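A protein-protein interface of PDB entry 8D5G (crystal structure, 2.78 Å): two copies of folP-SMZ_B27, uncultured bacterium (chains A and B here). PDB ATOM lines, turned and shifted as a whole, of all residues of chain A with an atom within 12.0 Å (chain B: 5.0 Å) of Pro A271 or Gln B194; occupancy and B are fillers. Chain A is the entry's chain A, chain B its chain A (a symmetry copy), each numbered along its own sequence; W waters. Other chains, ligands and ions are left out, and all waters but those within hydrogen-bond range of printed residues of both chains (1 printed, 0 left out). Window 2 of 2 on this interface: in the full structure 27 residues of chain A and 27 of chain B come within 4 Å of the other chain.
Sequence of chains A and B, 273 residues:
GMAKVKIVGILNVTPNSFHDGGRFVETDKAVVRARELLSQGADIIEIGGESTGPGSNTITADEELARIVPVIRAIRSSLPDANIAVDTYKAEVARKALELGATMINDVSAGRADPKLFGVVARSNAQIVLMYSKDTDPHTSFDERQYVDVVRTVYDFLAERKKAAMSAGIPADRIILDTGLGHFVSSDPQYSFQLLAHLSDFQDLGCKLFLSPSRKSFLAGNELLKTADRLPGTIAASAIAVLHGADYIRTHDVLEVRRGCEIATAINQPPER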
ATOM      1  N   GLY A   1       3.374 -39.358  25.660  1.00  0.00           N
ATOM      2  CA  GLY A   1       3.542 -38.721  26.954  1.00  0.00           C
ATOM      3  C   GLY A   1       4.787 -39.175  27.691  1.00  0.00           C
ATOM      4  O   GLY A   1       5.044 -40.372  27.807  1.00  0.00           O
ATOM      5  N   MET A   2       5.562 -38.213  28.192  1.00  0.00           N
ATOM      6  CA  MET A   2       6.791 -38.535  28.907  1.00  0.00           C
ATOM      7  C   MET A   2       6.481 -39.264  30.208  1.00  0.00           C
ATOM      8  O   MET A   2       5.605 -38.851  30.974  1.00  0.00           O
ATOM      9  CB  MET A   2       7.589 -37.262  29.190  1.00  0.00           C
ATOM     10  CG  MET A   2       8.707 -37.001  28.195  1.00  0.00           C
ATOM     11  SD  MET A   2       8.116 -36.326  26.632  1.00  0.00           S
ATOM     12  CE  MET A   2       8.344 -37.727  25.540  1.00  0.00           C
ATOM     13  N   LEU A 243      14.736 -33.070  35.061  1.00  0.00           N
ATOM     14  CA  LEU A 243      14.745 -32.271  33.840  1.00  0.00           C
ATOM     15  C   LEU A 243      15.951 -32.587  32.970  1.00  0.00           C
ATOM     16  O   LEU A 243      15.887 -32.441  31.744  1.00  0.00           O
ATOM     17  CB  LEU A 243      14.724 -30.782  34.183  1.00  0.00           C
ATOM     18  CG  LEU A 243      14.358 -29.831  33.039  1.00  0.00           C
ATOM     19  CD1 LEU A 243      12.857 -29.564  33.010  1.00  0.00           C
ATOM     20  CD2 LEU A 243      15.144 -28.532  33.145  1.00  0.00           C
ATOM     21  N   GLU A 262       7.337 -34.130  39.799  1.00  0.00           N
ATOM     22  CA  GLU A 262       6.188 -34.142  38.900  1.00  0.00           C
ATOM     23  C   GLU A 262       6.091 -32.842  38.113  1.00  0.00           C
ATOM     24  O   GLU A 262       5.664 -32.848  36.952  1.00  0.00           O
ATOM     25  CB  GLU A 262       4.902 -34.385  39.691  1.00  0.00           C
ATOM     26  CG  GLU A 262       3.701 -34.747  38.833  1.00  0.00           C
ATOM     27  CD  GLU A 262       2.382 -34.363  39.478  1.00  0.00           C
ATOM     28  OE1 GLU A 262       2.287 -34.418  40.723  1.00  0.00           O
ATOM     29  OE2 GLU A 262       1.438 -34.011  38.738  1.00  0.00           O
ATOM     30  N   ILE A 263       6.484 -31.724  38.725  1.00  0.00           N
ATOM     31  CA  ILE A 263       6.516 -30.458  38.003  1.00  0.00           C
ATOM     32  C   ILE A 263       7.586 -30.494  36.921  1.00  0.00           C
ATOM     33  O   ILE A 263       7.372 -30.012  35.801  1.00  0.00           O
ATOM     34  CB  ILE A 263       6.739 -29.292  38.984  1.00  0.00           C
ATOM     35  CG1 ILE A 263       5.668 -29.308  40.077  1.00  0.00           C
ATOM     36  CG2 ILE A 263       6.732 -27.962  38.244  1.00  0.00           C
ATOM     37  CD1 ILE A 263       4.259 -29.135  39.555  1.00  0.00           C
ATOM     38  N   ALA A 264       8.748 -31.075  37.230  1.00  0.00           N
ATOM     39  CA  ALA A 264       9.822 -31.158  36.246  1.00  0.00           C
ATOM     40  C   ALA A 264       9.420 -32.029  35.061  1.00  0.00           C
ATOM     41  O   ALA A 264       9.741 -31.711  33.910  1.00  0.00           O
ATOM     42  CB  ALA A 264      11.092 -31.697  36.902  1.00  0.00           C
ATOM     43  N   THR A 265       8.719 -33.135  35.324  1.00  0.00           N
ATOM     44  CA  THR A 265       8.252 -33.984  34.234  1.00  0.00           C
ATOM     45  C   THR A 265       7.226 -33.255  33.373  1.00  0.00           C
ATOM     46  O   THR A 265       7.218 -33.408  32.145  1.00  0.00           O
ATOM     47  CB  THR A 265       7.671 -35.284  34.794  1.00  0.00           C
ATOM     48  OG1 THR A 265       8.673 -35.961  35.564  1.00  0.00           O
ATOM     49  CG2 THR A 265       7.204 -36.198  33.669  1.00  0.00           C
ATOM     50  N   ALA A 266       6.366 -32.446  33.994  1.00  0.00           N
ATOM     51  CA  ALA A 266       5.393 -31.677  33.224  1.00  0.00           C
ATOM     52  C   ALA A 266       6.064 -30.597  32.386  1.00  0.00           C
ATOM     53  O   ALA A 266       5.576 -30.264  31.300  1.00  0.00           O
ATOM     54  CB  ALA A 266       4.353 -31.054  34.156  1.00  0.00           C
ATOM     55  N   ILE A 267       7.175 -30.036  32.870  1.00  0.00           N
ATOM     56  CA  ILE A 267       7.906 -29.055  32.075  1.00  0.00           C
ATOM     57  C   ILE A 267       8.603 -29.730  30.899  1.00  0.00           C
ATOM     58  O   ILE A 267       8.691 -29.156  29.806  1.00  0.00           O
ATOM     59  CB  ILE A 267       8.897 -28.282  32.967  1.00  0.00           C
ATOM     60  CG1 ILE A 267       8.138 -27.516  34.054  1.00  0.00           C
ATOM     61  CG2 ILE A 267       9.743 -27.328  32.140  1.00  0.00           C
ATOM     62  CD1 ILE A 267       9.028 -26.736  34.992  1.00  0.00           C
ATOM     63  N   ASN A 268       9.088 -30.959  31.090  1.00  0.00           N
ATOM     64  CA  ASN A 268       9.718 -31.711  30.012  1.00  0.00           C
ATOM     65  C   ASN A 268       8.718 -32.241  28.992  1.00  0.00           C
ATOM     66  O   ASN A 268       9.137 -32.715  27.930  1.00  0.00           O
ATOM     67  CB  ASN A 268      10.516 -32.881  30.589  1.00  0.00           C
ATOM     68  CG  ASN A 268      11.987 -32.564  30.748  1.00  0.00           C
ATOM     69  OD1 ASN A 268      12.492 -31.598  30.177  1.00  0.00           O
ATOM     70  ND2 ASN A 268      12.685 -33.380  31.528  1.00  0.00           N
ATOM     71  N   GLN A 269       7.421 -32.175  29.281  1.00  0.00           N
ATOM     72  CA  GLN A 269       6.411 -32.770  28.417  1.00  0.00           C
ATOM     73  C   GLN A 269       6.007 -31.784  27.330  1.00  0.00           C
ATOM     74  O   GLN A 269       5.466 -30.716  27.651  1.00  0.00           O
ATOM     75  CB  GLN A 269       5.192 -33.179  29.225  1.00  0.00           C
ATOM     76  CG  GLN A 269       4.002 -33.616  28.385  1.00  0.00           C
ATOM     77  CD  GLN A 269       4.085 -35.071  27.971  1.00  0.00           C
ATOM     78  OE1 GLN A 269       4.420 -35.940  28.777  1.00  0.00           O
ATOM     79  NE2 GLN A 269       3.776 -35.347  26.709  1.00  0.00           N
ATOM     80  N   PRO A 270       6.241 -32.087  26.057  1.00  0.00           N
ATOM     81  CA  PRO A 270       5.763 -31.217  24.981  1.00  0.00           C
ATOM     82  C   PRO A 270       4.248 -31.258  24.896  1.00  0.00           C
ATOM     83  O   PRO A 270       3.615 -32.173  25.444  1.00  0.00           O
ATOM     84  CB  PRO A 270       6.413 -31.819  23.726  1.00  0.00           C
ATOM     85  CG  PRO A 270       6.653 -33.246  24.079  1.00  0.00           C
ATOM     86  CD  PRO A 270       6.976 -33.254  25.542  1.00  0.00           C
ATOM     87  N   PRO A 271       3.628 -30.283  24.229  1.00  0.00           N
ATOM     88  CA  PRO A 271       2.164 -30.269  24.145  1.00  0.00           C
ATOM     89  C   PRO A 271       1.624 -31.505  23.443  1.00  0.00           C
ATOM     90  O   PRO A 271       2.315 -32.176  22.673  1.00  0.00           O
ATOM     91  CB  PRO A 271       1.862 -28.998  23.339  1.00  0.00           C
ATOM     92  CG  PRO A 271       3.150 -28.637  22.669  1.00  0.00           C
ATOM     93  CD  PRO A 271       4.229 -29.099  23.595  1.00  0.00           C
ATOM     94  N   GLU A 272       0.353 -31.796  23.718  1.00  0.00           N
ATOM     95  CA  GLU A 272      -0.375 -32.902  23.102  1.00  0.00           C
ATOM     96  C   GLU A 272      -0.629 -32.690  21.623  1.00  0.00           C
ATOM     97  O   GLU A 272      -1.384 -33.493  21.058  1.00  0.00           O
ATOM     98  CB  GLU A 272      -1.703 -33.118  23.827  1.00  0.00           C
ATOM     99  CG  GLU A 272      -1.618 -34.073  25.007  1.00  0.00           C
ATOM    100  CD  GLU A 272      -2.246 -35.425  24.720  1.00  0.00           C
ATOM    101  OE1 GLU A 272      -1.971 -35.998  23.644  1.00  0.00           O
ATOM    102  OE2 GLU A 272      -3.014 -35.918  25.573  1.00  0.00           O
ATOM    103  N   ARG A 273      -0.034 -31.655  21.035  1.00  0.00           N
ATOM    104  CA  ARG A 273      -0.151 -31.359  19.611  1.00  0.00           C
ATOM    105  C   ARG A 273      -1.602 -31.117  19.203  1.00  0.00           C
ATOM    106  O   ARG A 273      -2.151 -31.825  18.360  1.00  0.00           O
ATOM    107  CB  ARG A 273       0.456 -32.491  18.778  1.00  0.00           C
ATOM    108  CG  ARG A 273       1.873 -32.210  18.301  1.00  0.00           C
ATOM    109  CD  ARG A 273       1.870 -31.702  16.861  1.00  0.00           C
ATOM    110  NE  ARG A 273       3.018 -30.902  16.423  1.00  0.00           N
ATOM    111  CZ  ARG A 273       3.728 -30.041  17.150  1.00  0.00           C
ATOM    112  NH1 ARG A 273       3.411 -29.742  18.401  1.00  0.00           N
ATOM    113  NH2 ARG A 273       4.776 -29.440  16.593  1.00  0.00           N
ATOM    114  OXT ARG A 273      -2.252 -30.199  19.705  1.00  0.00           O
ATOM    115  N   VAL B 150       1.590 -21.339  22.517  1.00  0.00           N
ATOM    116  CA  VAL B 150       1.542 -20.284  23.525  1.00  0.00           C
ATOM    117  C   VAL B 150       2.838 -19.486  23.543  1.00  0.00           C
ATOM    118  O   VAL B 150       2.842 -18.303  23.906  1.00  0.00           O
ATOM    119  CB  VAL B 150       1.224 -20.883  24.912  1.00  0.00           C
ATOM    120  CG1 VAL B 150       2.369 -21.760  25.401  1.00  0.00           C
ATOM    121  CG2 VAL B 150       0.916 -19.785  25.917  1.00  0.00           C
ATOM    122  N   VAL B 151       3.950 -20.100  23.134  1.00  0.00           N
ATOM    123  CA  VAL B 151       5.235 -19.410  23.191  1.00  0.00           C
ATOM    124  C   VAL B 151       5.280 -18.269  22.183  1.00  0.00           C
ATOM    125  O   VAL B 151       5.739 -17.165  22.499  1.00  0.00           O
ATOM    126  CB  VAL B 151       6.388 -20.408  22.976  1.00  0.00           C
ATOM    127  CG1 VAL B 151       7.723 -19.682  22.975  1.00  0.00           C
ATOM    128  CG2 VAL B 151       6.361 -21.482  24.050  1.00  0.00           C
ATOM    129  N   GLN B 190      -1.220 -26.755  31.087  1.00  0.00           N
ATOM    130  CA  GLN B 190      -0.170 -27.166  30.161  1.00  0.00           C
ATOM    131  C   GLN B 190       0.625 -25.977  29.636  1.00  0.00           C
ATOM    132  O   GLN B 190       1.822 -26.107  29.358  1.00  0.00           O
ATOM    133  CB  GLN B 190      -0.773 -27.950  28.993  1.00  0.00           C
ATOM    134  CG  GLN B 190      -1.591 -27.108  28.018  1.00  0.00           C
ATOM    135  CD  GLN B 190      -1.977 -27.869  26.761  1.00  0.00           C
ATOM    136  OE1 GLN B 190      -1.116 -28.340  26.016  1.00  0.00           O
ATOM    137  NE2 GLN B 190      -3.277 -27.987  26.518  1.00  0.00           N
ATOM    138  N   TYR B 191      -0.011 -24.811  29.515  1.00  0.00           N
ATOM    139  CA  TYR B 191       0.641 -23.680  28.870  1.00  0.00           C
ATOM    140  C   TYR B 191       1.613 -22.966  29.800  1.00  0.00           C
ATOM    141  O   TYR B 191       2.609 -22.403  29.330  1.00  0.00           O
ATOM    142  CB  TYR B 191      -0.418 -22.716  28.335  1.00  0.00           C
ATOM    143  CG  TYR B 191      -1.301 -23.351  27.283  1.00  0.00           C
ATOM    144  CD1 TYR B 191      -0.786 -23.701  26.040  1.00  0.00           C
ATOM    145  CD2 TYR B 191      -2.640 -23.621  27.537  1.00  0.00           C
ATOM    146  CE1 TYR B 191      -1.584 -24.288  25.075  1.00  0.00           C
ATOM    147  CE2 TYR B 191      -3.445 -24.209  26.576  1.00  0.00           C
ATOM    148  CZ  TYR B 191      -2.910 -24.540  25.348  1.00  0.00           C
ATOM    149  OH  TYR B 191      -3.704 -25.123  24.387  1.00  0.00           O
ATOM    150  N   SER B 192       1.354 -22.978  31.110  1.00  0.00           N
ATOM    151  CA  SER B 192       2.344 -22.458  32.047  1.00  0.00           C
ATOM    152  C   SER B 192       3.593 -23.328  32.066  1.00  0.00           C
ATOM    153  O   SER B 192       4.707 -22.812  32.222  1.00  0.00           O
ATOM    154  CB  SER B 192       1.747 -22.350  33.450  1.00  0.00           C
ATOM    155  OG  SER B 192       0.433 -21.821  33.410  1.00  0.00           O
ATOM    156  N   PHE B 193       3.430 -24.645  31.898  1.00  0.00           N
ATOM    157  CA  PHE B 193       4.582 -25.538  31.840  1.00  0.00           C
ATOM    158  C   PHE B 193       5.376 -25.331  30.555  1.00  0.00           C
ATOM    159  O   PHE B 193       6.612 -25.343  30.574  1.00  0.00           O
ATOM    160  CB  PHE B 193       4.126 -26.991  31.953  1.00  0.00           C
ATOM    161  CG  PHE B 193       3.604 -27.358  33.310  1.00  0.00           C
ATOM    162  CD1 PHE B 193       4.326 -27.050  34.451  1.00  0.00           C
ATOM    163  CD2 PHE B 193       2.392 -28.016  33.446  1.00  0.00           C
ATOM    164  CE1 PHE B 193       3.850 -27.389  35.703  1.00  0.00           C
ATOM    165  CE2 PHE B 193       1.907 -28.357  34.696  1.00  0.00           C
ATOM    166  CZ  PHE B 193       2.638 -28.042  35.825  1.00  0.00           C
ATOM    167  N   GLN B 194       4.682 -25.149  29.429  1.00  0.00           N
ATOM    168  CA  GLN B 194       5.376 -24.934  28.164  1.00  0.00           C
ATOM    169  C   GLN B 194       6.155 -23.624  28.168  1.00  0.00           C
ATOM    170  O   GLN B 194       7.240 -23.547  27.581  1.00  0.00           O
ATOM    171  CB  GLN B 194       4.375 -24.963  27.007  1.00  0.00           C
ATOM    172  CG  GLN B 194       3.744 -26.327  26.776  1.00  0.00           C
ATOM    173  CD  GLN B 194       2.452 -26.248  25.985  1.00  0.00           C
ATOM    174  OE1 GLN B 194       2.329 -25.454  25.052  1.00  0.00           O
ATOM    175  NE2 GLN B 194       1.479 -27.074  26.356  1.00  0.00           N
ATOM    176  N   LEU B 195       5.626 -22.592  28.829  1.00  0.00           N
ATOM    177  CA  LEU B 195       6.356 -21.333  28.936  1.00  0.00           C
ATOM    178  C   LEU B 195       7.610 -21.495  29.787  1.00  0.00           C
ATOM    179  O   LEU B 195       8.660 -20.923  29.470  1.00  0.00           O
ATOM    180  CB  LEU B 195       5.450 -20.249  29.517  1.00  0.00           C
ATOM    181  CG  LEU B 195       4.377 -19.692  28.580  1.00  0.00           C
ATOM    182  CD1 LEU B 195       3.467 -18.731  29.328  1.00  0.00           C
ATOM    183  CD2 LEU B 195       5.010 -19.014  27.373  1.00  0.00           C
ATOM    184  N   LEU B 196       7.521 -22.271  30.871  1.00  0.00           N
ATOM    185  CA  LEU B 196       8.697 -22.531  31.695  1.00  0.00           C
ATOM    186  C   LEU B 196       9.751 -23.310  30.919  1.00  0.00           C
ATOM    187  O   LEU B 196      10.954 -23.072  31.079  1.00  0.00           O
ATOM    188  CB  LEU B 196       8.297 -23.291  32.959  1.00  0.00           C
ATOM    189  CG  LEU B 196       7.515 -22.524  34.024  1.00  0.00           C
ATOM    190  CD1 LEU B 196       6.970 -23.480  35.075  1.00  0.00           C
ATOM    191  CD2 LEU B 196       8.391 -21.463  34.668  1.00  0.00           C
ATOM    192  N   ALA B 197       9.319 -24.247  30.071  1.00  0.00           N
ATOM    193  CA  ALA B 197      10.270 -25.050  29.309  1.00  0.00           C
ATOM    194  C   ALA B 197      11.034 -24.199  28.304  1.00  0.00           C
ATOM    195  O   ALA B 197      12.243 -24.384  28.116  1.00  0.00           O
ATOM    196  CB  ALA B 197       9.542 -26.192  28.602  1.00  0.00           C
ATOM    197  N   HIS B 198      10.352 -23.256  27.656  1.00  0.00           N
ATOM    198  CA  HIS B 198      10.949 -22.409  26.631  1.00  0.00           C
ATOM    199  C   HIS B 198      11.169 -20.981  27.123  1.00  0.00           C
ATOM    200  O   HIS B 198      11.058 -20.029  26.349  1.00  0.00           O
ATOM    201  CB  HIS B 198      10.086 -22.410  25.371  1.00  0.00           C
ATOM    202  CG  HIS B 198       9.748 -23.779  24.873  1.00  0.00           C
ATOM    203  ND1 HIS B 198      10.632 -24.544  24.144  1.00  0.00           N
ATOM    204  CD2 HIS B 198       8.622 -24.521  24.997  1.00  0.00           C
ATOM    205  CE1 HIS B 198      10.067 -25.699  23.842  1.00  0.00           C
ATOM    206  NE2 HIS B 198       8.847 -25.711  24.348  1.00  0.00           N
HETATM  207  O   HOH W   1       2.699 -29.786  27.970  1.00  0.00           O
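NE2 of Gln B194 lies within hydrogen-bond range of OE1 of Gln B190 (2.9 Å).
Ile A263 touches Phe B193 (CG2 to CE1, 3.9 Å). Ala A266 touches Phe B193. Phe B193 touches Ile A267. Ile A267 touches Leu B196 (CD1 to CD1, 3.9 Å). Ala B197 touches Ile A267. Pro A271 touches Gln B194 (CB to NE2, 3.6 Å).
Of the 15 printed residues of chain A, 4 touch a printed residue of chain B. Hydrophobic or aromatic side chains of chain A that line the printed part of chain B: Ile A263, Ala A266, Ile A267 and Pro A271. Among the printed residues, 6 pairs touch across the chains. Among the printed residues, no Asp or Glu carboxylate lies within 4 Å of a Lys or Arg side-chain nitrogen of the other chain.
No position is printed for both chains. Of the 6 pairs that touch across the chains among the printed residues, none has its exchanged pair printed and touching as well.
Val B150 touches none of the printed residues of chain A. No residue of chain A comes within 4 Å of Ser B192. Of chain A, only Ile A263 (3.9 Å), Ala A266 (3.6 Å) and Ile A267 (3.9 Å) come within 4 Å of Phe B193. No residue of chain A comes within 4 Å of Leu B195. Printed residues of chain A within 4 Å of Leu B196: Ile A267 (3.9 Å). Ala B197 touches one residue of chain A. No residue of chain A comes within 4 Å of His B198. Of the printed residues of chain B, Ala A266 touches Phe B193. Printed residues of chain B within 4 Å of Ile A263: Phe B193 (3.9 Å). Printed residues of chain B within 4 Å of Ile A267: Phe B193 (3.9 Å), Leu B196 (3.9 Å) and Ala B197 (3.3 Å). Val B151 touches none of the printed residues of chain A. Glu A262 touches none of the printed residues of chain B. The nearest residue of chain A that does not touch Gln B194 is Gln A269 (4.8 Å). The nearest printed residue of chain B that does not touch Ala A266 is Gln B194 (5.5 Å).
Water W1 bridges the backbone carbonyl oxygen of Gln A269 (2.9 Å) and the side-chain amide nitrogen of Gln B194 (3.4 Å).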
